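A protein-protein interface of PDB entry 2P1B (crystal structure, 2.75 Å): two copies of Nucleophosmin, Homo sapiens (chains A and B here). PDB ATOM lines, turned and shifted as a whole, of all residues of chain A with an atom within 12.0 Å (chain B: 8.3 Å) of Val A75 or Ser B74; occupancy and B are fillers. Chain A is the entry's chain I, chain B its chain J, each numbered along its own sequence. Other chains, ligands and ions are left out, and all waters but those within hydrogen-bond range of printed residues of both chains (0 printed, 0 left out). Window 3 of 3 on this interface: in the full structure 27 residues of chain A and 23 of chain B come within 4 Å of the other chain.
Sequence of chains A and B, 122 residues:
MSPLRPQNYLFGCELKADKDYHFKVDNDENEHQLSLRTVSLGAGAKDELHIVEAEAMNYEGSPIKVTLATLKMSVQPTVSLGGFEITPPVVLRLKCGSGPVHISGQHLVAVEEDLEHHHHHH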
ATOM      1  N   VAL A  39     -22.169   0.728  21.437  1.00  0.00           N
ATOM      2  CA  VAL A  39     -22.041  -0.239  22.516  1.00  0.00           C
ATOM      3  C   VAL A  39     -20.594  -0.710  22.374  1.00  0.00           C
ATOM      4  O   VAL A  39     -20.174  -1.122  21.292  1.00  0.00           O
ATOM      5  CB  VAL A  39     -22.967  -1.436  22.320  1.00  0.00           C
ATOM      6  CG1 VAL A  39     -22.823  -2.392  23.485  1.00  0.00           C
ATOM      7  CG2 VAL A  39     -24.398  -0.962  22.188  1.00  0.00           C
ATOM      8  N   SER A  40     -19.829  -0.639  23.454  1.00  0.00           N
ATOM      9  CA  SER A  40     -18.430  -1.032  23.393  1.00  0.00           C
ATOM     10  C   SER A  40     -17.860  -1.557  24.713  1.00  0.00           C
ATOM     11  O   SER A  40     -18.349  -1.230  25.794  1.00  0.00           O
ATOM     12  CB  SER A  40     -17.600   0.155  22.883  1.00  0.00           C
ATOM     13  OG  SER A  40     -18.257   1.386  23.146  1.00  0.00           O
ATOM     14  N   LEU A  41     -16.825  -2.385  24.607  1.00  0.00           N
ATOM     15  CA  LEU A  41     -16.173  -2.963  25.765  1.00  0.00           C
ATOM     16  C   LEU A  41     -15.220  -1.968  26.400  1.00  0.00           C
ATOM     17  O   LEU A  41     -14.728  -1.058  25.745  1.00  0.00           O
ATOM     18  CB  LEU A  41     -15.414  -4.220  25.361  1.00  0.00           C
ATOM     19  CG  LEU A  41     -16.330  -5.330  24.848  1.00  0.00           C
ATOM     20  CD1 LEU A  41     -15.506  -6.534  24.419  1.00  0.00           C
ATOM     21  CD2 LEU A  41     -17.329  -5.703  25.943  1.00  0.00           C
ATOM     22  N   ALA A  45     -12.890  -5.952  31.148  1.00  0.00           N
ATOM     23  CA  ALA A  45     -13.525  -6.908  30.243  1.00  0.00           C
ATOM     24  C   ALA A  45     -12.601  -7.940  29.627  1.00  0.00           C
ATOM     25  O   ALA A  45     -11.838  -7.633  28.716  1.00  0.00           O
ATOM     26  CB  ALA A  45     -14.251  -6.151  29.131  1.00  0.00           C
ATOM     27  N   LYS A  46     -12.679  -9.173  30.114  1.00  0.00           N
ATOM     28  CA  LYS A  46     -11.851 -10.238  29.567  1.00  0.00           C
ATOM     29  C   LYS A  46     -12.404 -10.535  28.176  1.00  0.00           C
ATOM     30  O   LYS A  46     -13.569 -10.252  27.886  1.00  0.00           O
ATOM     31  CB  LYS A  46     -11.942 -11.501  30.422  1.00  0.00           C
ATOM     32  CG  LYS A  46     -12.272 -11.264  31.882  1.00  0.00           C
ATOM     33  CD  LYS A  46     -12.512 -12.582  32.608  1.00  0.00           C
ATOM     34  CE  LYS A  46     -11.217 -13.327  32.904  1.00  0.00           C
ATOM     35  NZ  LYS A  46     -10.783 -13.129  34.319  1.00  0.00           N
ATOM     36  N   ASP A  47     -11.571 -11.115  27.322  1.00  0.00           N
ATOM     37  CA  ASP A  47     -11.980 -11.429  25.961  1.00  0.00           C
ATOM     38  C   ASP A  47     -13.039 -12.527  25.863  1.00  0.00           C
ATOM     39  O   ASP A  47     -12.871 -13.495  25.123  1.00  0.00           O
ATOM     40  CB  ASP A  47     -10.751 -11.805  25.121  1.00  0.00           C
ATOM     41  CG  ASP A  47     -11.102 -12.120  23.678  1.00  0.00           C
ATOM     42  OD1 ASP A  47     -11.830 -11.316  23.059  1.00  0.00           O
ATOM     43  OD2 ASP A  47     -10.648 -13.166  23.163  1.00  0.00           O
ATOM     44  N   GLU A  48     -14.131 -12.388  26.605  1.00  0.00           N
ATOM     45  CA  GLU A  48     -15.194 -13.378  26.530  1.00  0.00           C
ATOM     46  C   GLU A  48     -16.402 -12.771  25.839  1.00  0.00           C
ATOM     47  O   GLU A  48     -16.499 -11.544  25.722  1.00  0.00           O
ATOM     48  CB  GLU A  48     -15.584 -13.877  27.920  1.00  0.00           C
ATOM     49  CG  GLU A  48     -15.759 -12.799  28.962  1.00  0.00           C
ATOM     50  CD  GLU A  48     -16.558 -13.295  30.147  1.00  0.00           C
ATOM     51  OE1 GLU A  48     -16.538 -12.622  31.197  1.00  0.00           O
ATOM     52  OE2 GLU A  48     -17.215 -14.352  30.022  1.00  0.00           O
ATOM     53  N   LEU A  49     -17.320 -13.625  25.386  1.00  0.00           N
ATOM     54  CA  LEU A  49     -18.513 -13.148  24.692  1.00  0.00           C
ATOM     55  C   LEU A  49     -19.246 -12.090  25.505  1.00  0.00           C
ATOM     56  O   LEU A  49     -19.125 -12.028  26.727  1.00  0.00           O
ATOM     57  CB  LEU A  49     -19.472 -14.294  24.381  1.00  0.00           C
ATOM     58  CG  LEU A  49     -20.487 -13.923  23.298  1.00  0.00           C
ATOM     59  CD1 LEU A  49     -19.795 -13.848  21.945  1.00  0.00           C
ATOM     60  CD2 LEU A  49     -21.585 -14.956  23.258  1.00  0.00           C
ATOM     61  N   HIS A  50     -20.013 -11.259  24.814  1.00  0.00           N
ATOM     62  CA  HIS A  50     -20.745 -10.176  25.453  1.00  0.00           C
ATOM     63  C   HIS A  50     -22.037  -9.857  24.733  1.00  0.00           C
ATOM     64  O   HIS A  50     -22.049  -9.554  23.540  1.00  0.00           O
ATOM     65  CB  HIS A  50     -19.880  -8.922  25.483  1.00  0.00           C
ATOM     66  CG  HIS A  50     -19.043  -8.801  26.713  1.00  0.00           C
ATOM     67  ND1 HIS A  50     -19.497  -8.176  27.853  1.00  0.00           N
ATOM     68  CD2 HIS A  50     -17.791  -9.233  26.991  1.00  0.00           C
ATOM     69  CE1 HIS A  50     -18.560  -8.226  28.780  1.00  0.00           C
ATOM     70  NE2 HIS A  50     -17.513  -8.860  28.284  1.00  0.00           N
ATOM     71  N   ALA A  69     -26.710  -5.867  21.013  1.00  0.00           N
ATOM     72  CA  ALA A  69     -25.492  -6.311  20.346  1.00  0.00           C
ATOM     73  C   ALA A  69     -24.749  -7.453  21.036  1.00  0.00           C
ATOM     74  O   ALA A  69     -24.909  -7.696  22.230  1.00  0.00           O
ATOM     75  CB  ALA A  69     -24.544  -5.127  20.177  1.00  0.00           C
ATOM     76  N   THR A  70     -23.927  -8.145  20.252  1.00  0.00           N
ATOM     77  CA  THR A  70     -23.097  -9.234  20.739  1.00  0.00           C
ATOM     78  C   THR A  70     -21.664  -8.796  20.449  1.00  0.00           C
ATOM     79  O   THR A  70     -21.257  -8.701  19.295  1.00  0.00           O
ATOM     80  CB  THR A  70     -23.406 -10.539  20.002  1.00  0.00           C
ATOM     81  OG1 THR A  70     -24.678 -11.026  20.436  1.00  0.00           O
ATOM     82  CG2 THR A  70     -22.341 -11.586  20.283  1.00  0.00           C
ATOM     83  N   LEU A  71     -20.919  -8.515  21.513  1.00  0.00           N
ATOM     84  CA  LEU A  71     -19.537  -8.051  21.417  1.00  0.00           C
ATOM     85  C   LEU A  71     -18.497  -9.059  21.888  1.00  0.00           C
ATOM     86  O   LEU A  71     -18.795  -9.984  22.627  1.00  0.00           O
ATOM     87  CB  LEU A  71     -19.365  -6.786  22.255  1.00  0.00           C
ATOM     88  CG  LEU A  71     -20.120  -5.514  21.883  1.00  0.00           C
ATOM     89  CD1 LEU A  71     -20.436  -4.725  23.136  1.00  0.00           C
ATOM     90  CD2 LEU A  71     -19.277  -4.685  20.925  1.00  0.00           C
ATOM     91  N   LYS A  72     -17.264  -8.861  21.446  1.00  0.00           N
ATOM     92  CA  LYS A  72     -16.141  -9.699  21.849  1.00  0.00           C
ATOM     93  C   LYS A  72     -14.903  -8.871  21.567  1.00  0.00           C
ATOM     94  O   LYS A  72     -14.719  -8.366  20.460  1.00  0.00           O
ATOM     95  CB  LYS A  72     -16.086 -11.022  21.079  1.00  0.00           C
ATOM     96  CG  LYS A  72     -15.125 -12.038  21.722  1.00  0.00           C
ATOM     97  CD  LYS A  72     -15.203 -13.423  21.077  1.00  0.00           C
ATOM     98  CE  LYS A  72     -14.345 -14.432  21.822  1.00  0.00           C
ATOM     99  NZ  LYS A  72     -12.903 -14.056  21.817  1.00  0.00           N
ATOM    100  N   MET A  73     -14.065  -8.730  22.587  1.00  0.00           N
ATOM    101  CA  MET A  73     -12.862  -7.920  22.507  1.00  0.00           C
ATOM    102  C   MET A  73     -11.896  -8.255  21.380  1.00  0.00           C
ATOM    103  O   MET A  73     -11.419  -7.357  20.689  1.00  0.00           O
ATOM    104  CB  MET A  73     -12.124  -7.994  23.840  1.00  0.00           C
ATOM    105  CG  MET A  73     -11.013  -6.992  23.994  1.00  0.00           C
ATOM    106  SD  MET A  73     -11.610  -5.304  23.940  1.00  0.00           S
ATOM    107  CE  MET A  73     -12.122  -5.051  25.624  1.00  0.00           C
ATOM    108  N   SER A  74     -11.599  -9.540  21.200  1.00  0.00           N
ATOM    109  CA  SER A  74     -10.661  -9.976  20.163  1.00  0.00           C
ATOM    110  C   SER A  74     -11.244  -9.991  18.766  1.00  0.00           C
ATOM    111  O   SER A  74     -10.513 -10.220  17.807  1.00  0.00           O
ATOM    112  CB  SER A  74     -10.087 -11.370  20.487  1.00  0.00           C
ATOM    113  OG  SER A  74     -11.091 -12.366  20.611  1.00  0.00           O
ATOM    114  N   VAL A  75     -12.548  -9.754  18.649  1.00  0.00           N
ATOM    115  CA  VAL A  75     -13.195  -9.751  17.343  1.00  0.00           C
ATOM    116  C   VAL A  75     -13.849  -8.435  16.973  1.00  0.00           C
ATOM    117  O   VAL A  75     -13.529  -7.841  15.958  1.00  0.00           O
ATOM    118  CB  VAL A  75     -14.281 -10.823  17.241  1.00  0.00           C
ATOM    119  CG1 VAL A  75     -14.954 -10.731  15.884  1.00  0.00           C
ATOM    120  CG2 VAL A  75     -13.685 -12.192  17.444  1.00  0.00           C
ATOM    121  N   GLN A  76     -14.790  -7.997  17.791  1.00  0.00           N
ATOM    122  CA  GLN A  76     -15.498  -6.756  17.535  1.00  0.00           C
ATOM    123  C   GLN A  76     -15.786  -6.093  18.872  1.00  0.00           C
ATOM    124  O   GLN A  76     -16.732  -6.455  19.563  1.00  0.00           O
ATOM    125  CB  GLN A  76     -16.788  -7.067  16.785  1.00  0.00           C
ATOM    126  CG  GLN A  76     -17.748  -5.912  16.647  1.00  0.00           C
ATOM    127  CD  GLN A  76     -18.936  -6.266  15.775  1.00  0.00           C
ATOM    128  OE1 GLN A  76     -19.511  -7.352  15.899  1.00  0.00           O
ATOM    129  NE2 GLN A  76     -19.317  -5.349  14.892  1.00  0.00           N
ATOM    130  N   PRO A  77     -14.960  -5.114  19.256  1.00  0.00           N
ATOM    131  CA  PRO A  77     -15.110  -4.396  20.523  1.00  0.00           C
ATOM    132  C   PRO A  77     -16.215  -3.354  20.530  1.00  0.00           C
ATOM    133  O   PRO A  77     -16.654  -2.918  21.591  1.00  0.00           O
ATOM    134  CB  PRO A  77     -13.739  -3.750  20.720  1.00  0.00           C
ATOM    135  CG  PRO A  77     -12.829  -4.567  19.852  1.00  0.00           C
ATOM    136  CD  PRO A  77     -13.673  -4.779  18.638  1.00  0.00           C
ATOM    137  N   THR A  78     -16.667  -2.954  19.349  1.00  0.00           N
ATOM    138  CA  THR A  78     -17.692  -1.924  19.271  1.00  0.00           C
ATOM    139  C   THR A  78     -18.747  -2.152  18.213  1.00  0.00           C
ATOM    140  O   THR A  78     -18.454  -2.599  17.107  1.00  0.00           O
ATOM    141  CB  THR A  78     -17.061  -0.547  18.992  1.00  0.00           C
ATOM    142  OG1 THR A  78     -16.223  -0.164  20.092  1.00  0.00           O
ATOM    143  CG2 THR A  78     -18.145   0.504  18.789  1.00  0.00           C
ATOM    144  N   VAL A  79     -19.984  -1.834  18.571  1.00  0.00           N
ATOM    145  CA  VAL A  79     -21.107  -1.950  17.654  1.00  0.00           C
ATOM    146  C   VAL A  79     -21.763  -0.577  17.632  1.00  0.00           C
ATOM    147  O   VAL A  79     -22.022   0.012  18.686  1.00  0.00           O
ATOM    148  CB  VAL A  79     -22.137  -2.994  18.129  1.00  0.00           C
ATOM    149  CG1 VAL A  79     -23.318  -3.018  17.179  1.00  0.00           C
ATOM    150  CG2 VAL A  79     -21.505  -4.368  18.188  1.00  0.00           C
ATOM    151  N   SER A  80     -22.010  -0.059  16.433  1.00  0.00           N
ATOM    152  CA  SER A  80     -22.630   1.251  16.285  1.00  0.00           C
ATOM    153  C   SER A  80     -24.086   1.126  15.833  1.00  0.00           C
ATOM    154  O   SER A  80     -24.372   0.939  14.648  1.00  0.00           O
ATOM    155  CB  SER A  80     -21.840   2.093  15.279  1.00  0.00           C
ATOM    156  OG  SER A  80     -22.335   3.419  15.206  1.00  0.00           O
ATOM    157  N   LEU B  41     -25.476 -12.834  16.884  1.00  0.00           N
ATOM    158  CA  LEU B  41     -25.500 -14.221  17.346  1.00  0.00           C
ATOM    159  C   LEU B  41     -25.546 -14.229  18.857  1.00  0.00           C
ATOM    160  O   LEU B  41     -24.823 -13.475  19.500  1.00  0.00           O
ATOM    161  CB  LEU B  41     -24.247 -14.970  16.906  1.00  0.00           C
ATOM    162  CG  LEU B  41     -23.829 -14.769  15.457  1.00  0.00           C
ATOM    163  CD1 LEU B  41     -22.437 -15.312  15.291  1.00  0.00           C
ATOM    164  CD2 LEU B  41     -24.796 -15.446  14.511  1.00  0.00           C
ATOM    165  N   ALA B  45     -24.610 -19.923  19.944  1.00  0.00           N
ATOM    166  CA  ALA B  45     -24.398 -20.129  18.517  1.00  0.00           C
ATOM    167  C   ALA B  45     -23.091 -20.837  18.205  1.00  0.00           C
ATOM    168  O   ALA B  45     -22.054 -20.519  18.778  1.00  0.00           O
ATOM    169  CB  ALA B  45     -24.446 -18.790  17.784  1.00  0.00           C
ATOM    170  N   LYS B  46     -23.148 -21.805  17.298  1.00  0.00           N
ATOM    171  CA  LYS B  46     -21.952 -22.530  16.888  1.00  0.00           C
ATOM    172  C   LYS B  46     -21.188 -21.582  15.974  1.00  0.00           C
ATOM    173  O   LYS B  46     -21.805 -20.750  15.308  1.00  0.00           O
ATOM    174  CB  LYS B  46     -22.338 -23.811  16.135  1.00  0.00           C
ATOM    175  CG  LYS B  46     -22.953 -24.895  17.036  1.00  0.00           C
ATOM    176  CD  LYS B  46     -24.223 -25.514  16.438  1.00  0.00           C
ATOM    177  CE  LYS B  46     -23.938 -26.353  15.204  1.00  0.00           C
ATOM    178  NZ  LYS B  46     -23.147 -27.572  15.522  1.00  0.00           N
ATOM    179  N   ASP B  47     -19.861 -21.680  15.943  1.00  0.00           N
ATOM    180  CA  ASP B  47     -19.097 -20.779  15.088  1.00  0.00           C
ATOM    181  C   ASP B  47     -19.214 -21.160  13.628  1.00  0.00           C
ATOM    182  O   ASP B  47     -18.219 -21.323  12.931  1.00  0.00           O
ATOM    183  CB  ASP B  47     -17.617 -20.724  15.482  1.00  0.00           C
ATOM    184  CG  ASP B  47     -16.829 -19.718  14.637  1.00  0.00           C
ATOM    185  OD1 ASP B  47     -17.395 -18.660  14.283  1.00  0.00           O
ATOM    186  OD2 ASP B  47     -15.646 -19.977  14.332  1.00  0.00           O
ATOM    187  N   GLU B  48     -20.451 -21.309  13.178  1.00  0.00           N
ATOM    188  CA  GLU B  48     -20.722 -21.635  11.794  1.00  0.00           C
ATOM    189  C   GLU B  48     -21.248 -20.369  11.122  1.00  0.00           C
ATOM    190  O   GLU B  48     -21.477 -19.354  11.791  1.00  0.00           O
ATOM    191  CB  GLU B  48     -21.751 -22.761  11.717  1.00  0.00           C
ATOM    192  CG  GLU B  48     -22.970 -22.553  12.600  1.00  0.00           C
ATOM    193  CD  GLU B  48     -24.022 -23.640  12.415  1.00  0.00           C
ATOM    194  OE1 GLU B  48     -25.106 -23.513  13.015  1.00  0.00           O
ATOM    195  OE2 GLU B  48     -23.770 -24.619  11.673  1.00  0.00           O
ATOM    196  N   LEU B  71     -23.455 -13.618   9.030  1.00  0.00           N
ATOM    197  CA  LEU B  71     -22.665 -13.496  10.259  1.00  0.00           C
ATOM    198  C   LEU B  71     -21.846 -14.708  10.645  1.00  0.00           C
ATOM    199  O   LEU B  71     -22.208 -15.832  10.321  1.00  0.00           O
ATOM    200  CB  LEU B  71     -23.586 -13.158  11.430  1.00  0.00           C
ATOM    201  CG  LEU B  71     -24.461 -11.932  11.184  1.00  0.00           C
ATOM    202  CD1 LEU B  71     -25.901 -12.375  11.035  1.00  0.00           C
ATOM    203  CD2 LEU B  71     -24.307 -10.942  12.327  1.00  0.00           C
ATOM    204  N   LYS B  72     -20.735 -14.471  11.337  1.00  0.00           N
ATOM    205  CA  LYS B  72     -19.890 -15.561  11.819  1.00  0.00           C
ATOM    206  C   LYS B  72     -19.280 -15.181  13.166  1.00  0.00           C
ATOM    207  O   LYS B  72     -18.450 -14.280  13.265  1.00  0.00           O
ATOM    208  CB  LYS B  72     -18.800 -15.918  10.808  1.00  0.00           C
ATOM    209  CG  LYS B  72     -18.198 -17.290  11.084  1.00  0.00           C
ATOM    210  CD  LYS B  72     -17.289 -17.787   9.968  1.00  0.00           C
ATOM    211  CE  LYS B  72     -16.755 -19.177  10.295  1.00  0.00           C
ATOM    212  NZ  LYS B  72     -16.101 -19.191  11.640  1.00  0.00           N
ATOM    213  N   MET B  73     -19.710 -15.888  14.203  1.00  0.00           N
ATOM    214  CA  MET B  73     -19.288 -15.654  15.585  1.00  0.00           C
ATOM    215  C   MET B  73     -17.830 -15.244  15.830  1.00  0.00           C
ATOM    216  O   MET B  73     -17.551 -14.488  16.759  1.00  0.00           O
ATOM    217  CB  MET B  73     -19.630 -16.893  16.429  1.00  0.00           C
ATOM    218  CG  MET B  73     -19.280 -16.783  17.915  1.00  0.00           C
ATOM    219  SD  MET B  73     -20.149 -15.468  18.830  1.00  0.00           S
ATOM    220  CE  MET B  73     -21.724 -16.196  19.061  1.00  0.00           C
ATOM    221  N   SER B  74     -16.904 -15.729  15.009  1.00  0.00           N
ATOM    222  CA  SER B  74     -15.492 -15.397  15.205  1.00  0.00           C
ATOM    223  C   SER B  74     -14.992 -14.352  14.218  1.00  0.00           C
ATOM    224  O   SER B  74     -13.792 -14.112  14.129  1.00  0.00           O
ATOM    225  CB  SER B  74     -14.615 -16.654  15.085  1.00  0.00           C
ATOM    226  OG  SER B  74     -14.398 -17.016  13.728  1.00  0.00           O
ATOM    227  N   VAL B  75     -15.913 -13.738  13.480  1.00  0.00           N
ATOM    228  CA  VAL B  75     -15.563 -12.721  12.491  1.00  0.00           C
ATOM    229  C   VAL B  75     -16.488 -11.521  12.558  1.00  0.00           C
ATOM    230  O   VAL B  75     -16.042 -10.378  12.582  1.00  0.00           O
ATOM    231  CB  VAL B  75     -15.639 -13.271  11.063  1.00  0.00           C
ATOM    232  CG1 VAL B  75     -15.480 -12.133  10.066  1.00  0.00           C
ATOM    233  CG2 VAL B  75     -14.566 -14.320  10.859  1.00  0.00           C
ATOM    234  N   GLN B  76     -17.786 -11.783  12.563  1.00  0.00           N
ATOM    235  CA  GLN B  76     -18.752 -10.708  12.635  1.00  0.00           C
ATOM    236  C   GLN B  76     -19.985 -11.152  13.411  1.00  0.00           C
ATOM    237  O   GLN B  76     -21.003 -11.526  12.834  1.00  0.00           O
ATOM    238  CB  GLN B  76     -19.128 -10.234  11.228  1.00  0.00           C
ATOM    239  CG  GLN B  76     -19.902  -8.919  11.220  1.00  0.00           C
ATOM    240  CD  GLN B  76     -19.927  -8.240   9.854  1.00  0.00           C
ATOM    241  OE1 GLN B  76     -20.305  -8.843   8.850  1.00  0.00           O
ATOM    242  NE2 GLN B  76     -19.527  -6.972   9.820  1.00  0.00           N
ATOM    243  N   PRO B  77     -19.891 -11.138  14.742  1.00  0.00           N
ATOM    244  CA  PRO B  77     -21.002 -11.536  15.606  1.00  0.00           C
ATOM    245  C   PRO B  77     -22.175 -10.562  15.559  1.00  0.00           C
ATOM    246  O   PRO B  77     -23.211 -10.806  16.177  1.00  0.00           O
ATOM    247  CB  PRO B  77     -20.359 -11.594  16.989  1.00  0.00           C
ATOM    248  CG  PRO B  77     -19.267 -10.566  16.892  1.00  0.00           C
ATOM    249  CD  PRO B  77     -18.682 -10.884  15.540  1.00  0.00           C
ATOM    250  N   THR B  78     -22.022  -9.460  14.831  1.00  0.00           N
ATOM    251  CA  THR B  78     -23.110  -8.492  14.755  1.00  0.00           C
ATOM    252  C   THR B  78     -23.069  -7.555  13.561  1.00  0.00           C
ATOM    253  O   THR B  78     -22.058  -6.897  13.299  1.00  0.00           O
ATOM    254  CB  THR B  78     -23.164  -7.591  16.003  1.00  0.00           C
ATOM    255  OG1 THR B  78     -23.295  -8.392  17.185  1.00  0.00           O
ATOM    256  CG2 THR B  78     -24.350  -6.639  15.911  1.00  0.00           C
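OG1 of Thr A70 lies within hydrogen-bond range of O of Leu B41, 2.6 Å away. The backbone carbonyl oxygen (O) of Thr A70 lies within hydrogen-bond range of the side-chain hydroxyl (OG1) of Thr B78, 2.9 Å away. N of Thr B78 is in hydrogen-bond range of OE1 of Gln A76 (3.4 Å).
Printed residues of chain A that touch a printed residue of chain B: Leu A49, Thr A70, Val A75, Gln A76 and Val A79. Along chain A the printed residues that touch a printed residue of chain B span positions 49 to 79. Of the 13 printed residues of chain B, 6 touch a printed residue of chain A. Among the printed residues, no Asp or Glu carboxylate lies within 4 Å of a Lys or Arg side-chain nitrogen of the other chain.
Among the printed residues, pairs that only touch across the chains: Leu A49 with Met B73 (3.5 Å), Thr A70 with Pro B77 (3.6 Å), Val A75 with Ser B74 (3.8 Å), Val A75 with Val B75 (3.5 Å), Val A75 with Pro B77 (3.7 Å), Gln A76 with Pro B77 (3.4 Å) and Val A79 with Thr B78 (3.97 Å).
The backbone carbonyl oxygen of Val A39 sits at hydrogen-bond distance from the backbone NH of Val A79, 2.8 Å away. The backbone NH (N) of Leu B41 lies within hydrogen-bond range of the backbone carbonyl oxygen (O) of Pro B77, at 3.1 Å. The side-chain carboxylate (OD1) of Asp B47 sits at hydrogen-bond distance from the backbone NH (N) of Ser B74 (3.1 Å). NZ of Lys B72 lies within hydrogen-bond range of OG of Ser B74.
Of chain B, only Ser B74 (3.8 Å), Val B75 (3.5 Å) and Pro B77 (3.7 Å) come within 4 Å of Val A75. Printed residues of chain A within 4 Å of Ser B74: Val A75 (3.8 Å). No residue of chain B comes within 4 Å of Ser A74. No residue of chain A comes within 4 Å of Lys B72. Val B75 touches one residue of chain A. Of the printed residues of chain B, Thr A70 touches Leu B41, Pro B77 and Thr B78. Of the printed residues of chain A, Thr B78 touches Thr A70, Gln A76 and Val A79. Lys B46 touches none of the printed residues of chain A. Lys A72 touches none of the printed residues of chain B.
Val A75 touches its own counterpart, Val B75. Val A75 touches Pro B77, but with the chains exchanged Pro A77 does not touch Val B75 (8.6 Å). Gln A76 touches Pro B77, but with the chains exchanged Pro A77 does not touch Gln B76 (9.5 Å). Gln A76 touches Thr B78, but with the chains exchanged Thr A78 does not touch Gln B76 (8.6 Å). Positions printed for both chains: 41, 45, 46, 47, 48, 71, 72, 73, 74, 75, 76, 77 and 78. Of the 10 pairs that touch across the chains among the printed residues, 1 has its exchanged pair printed and touching as well.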
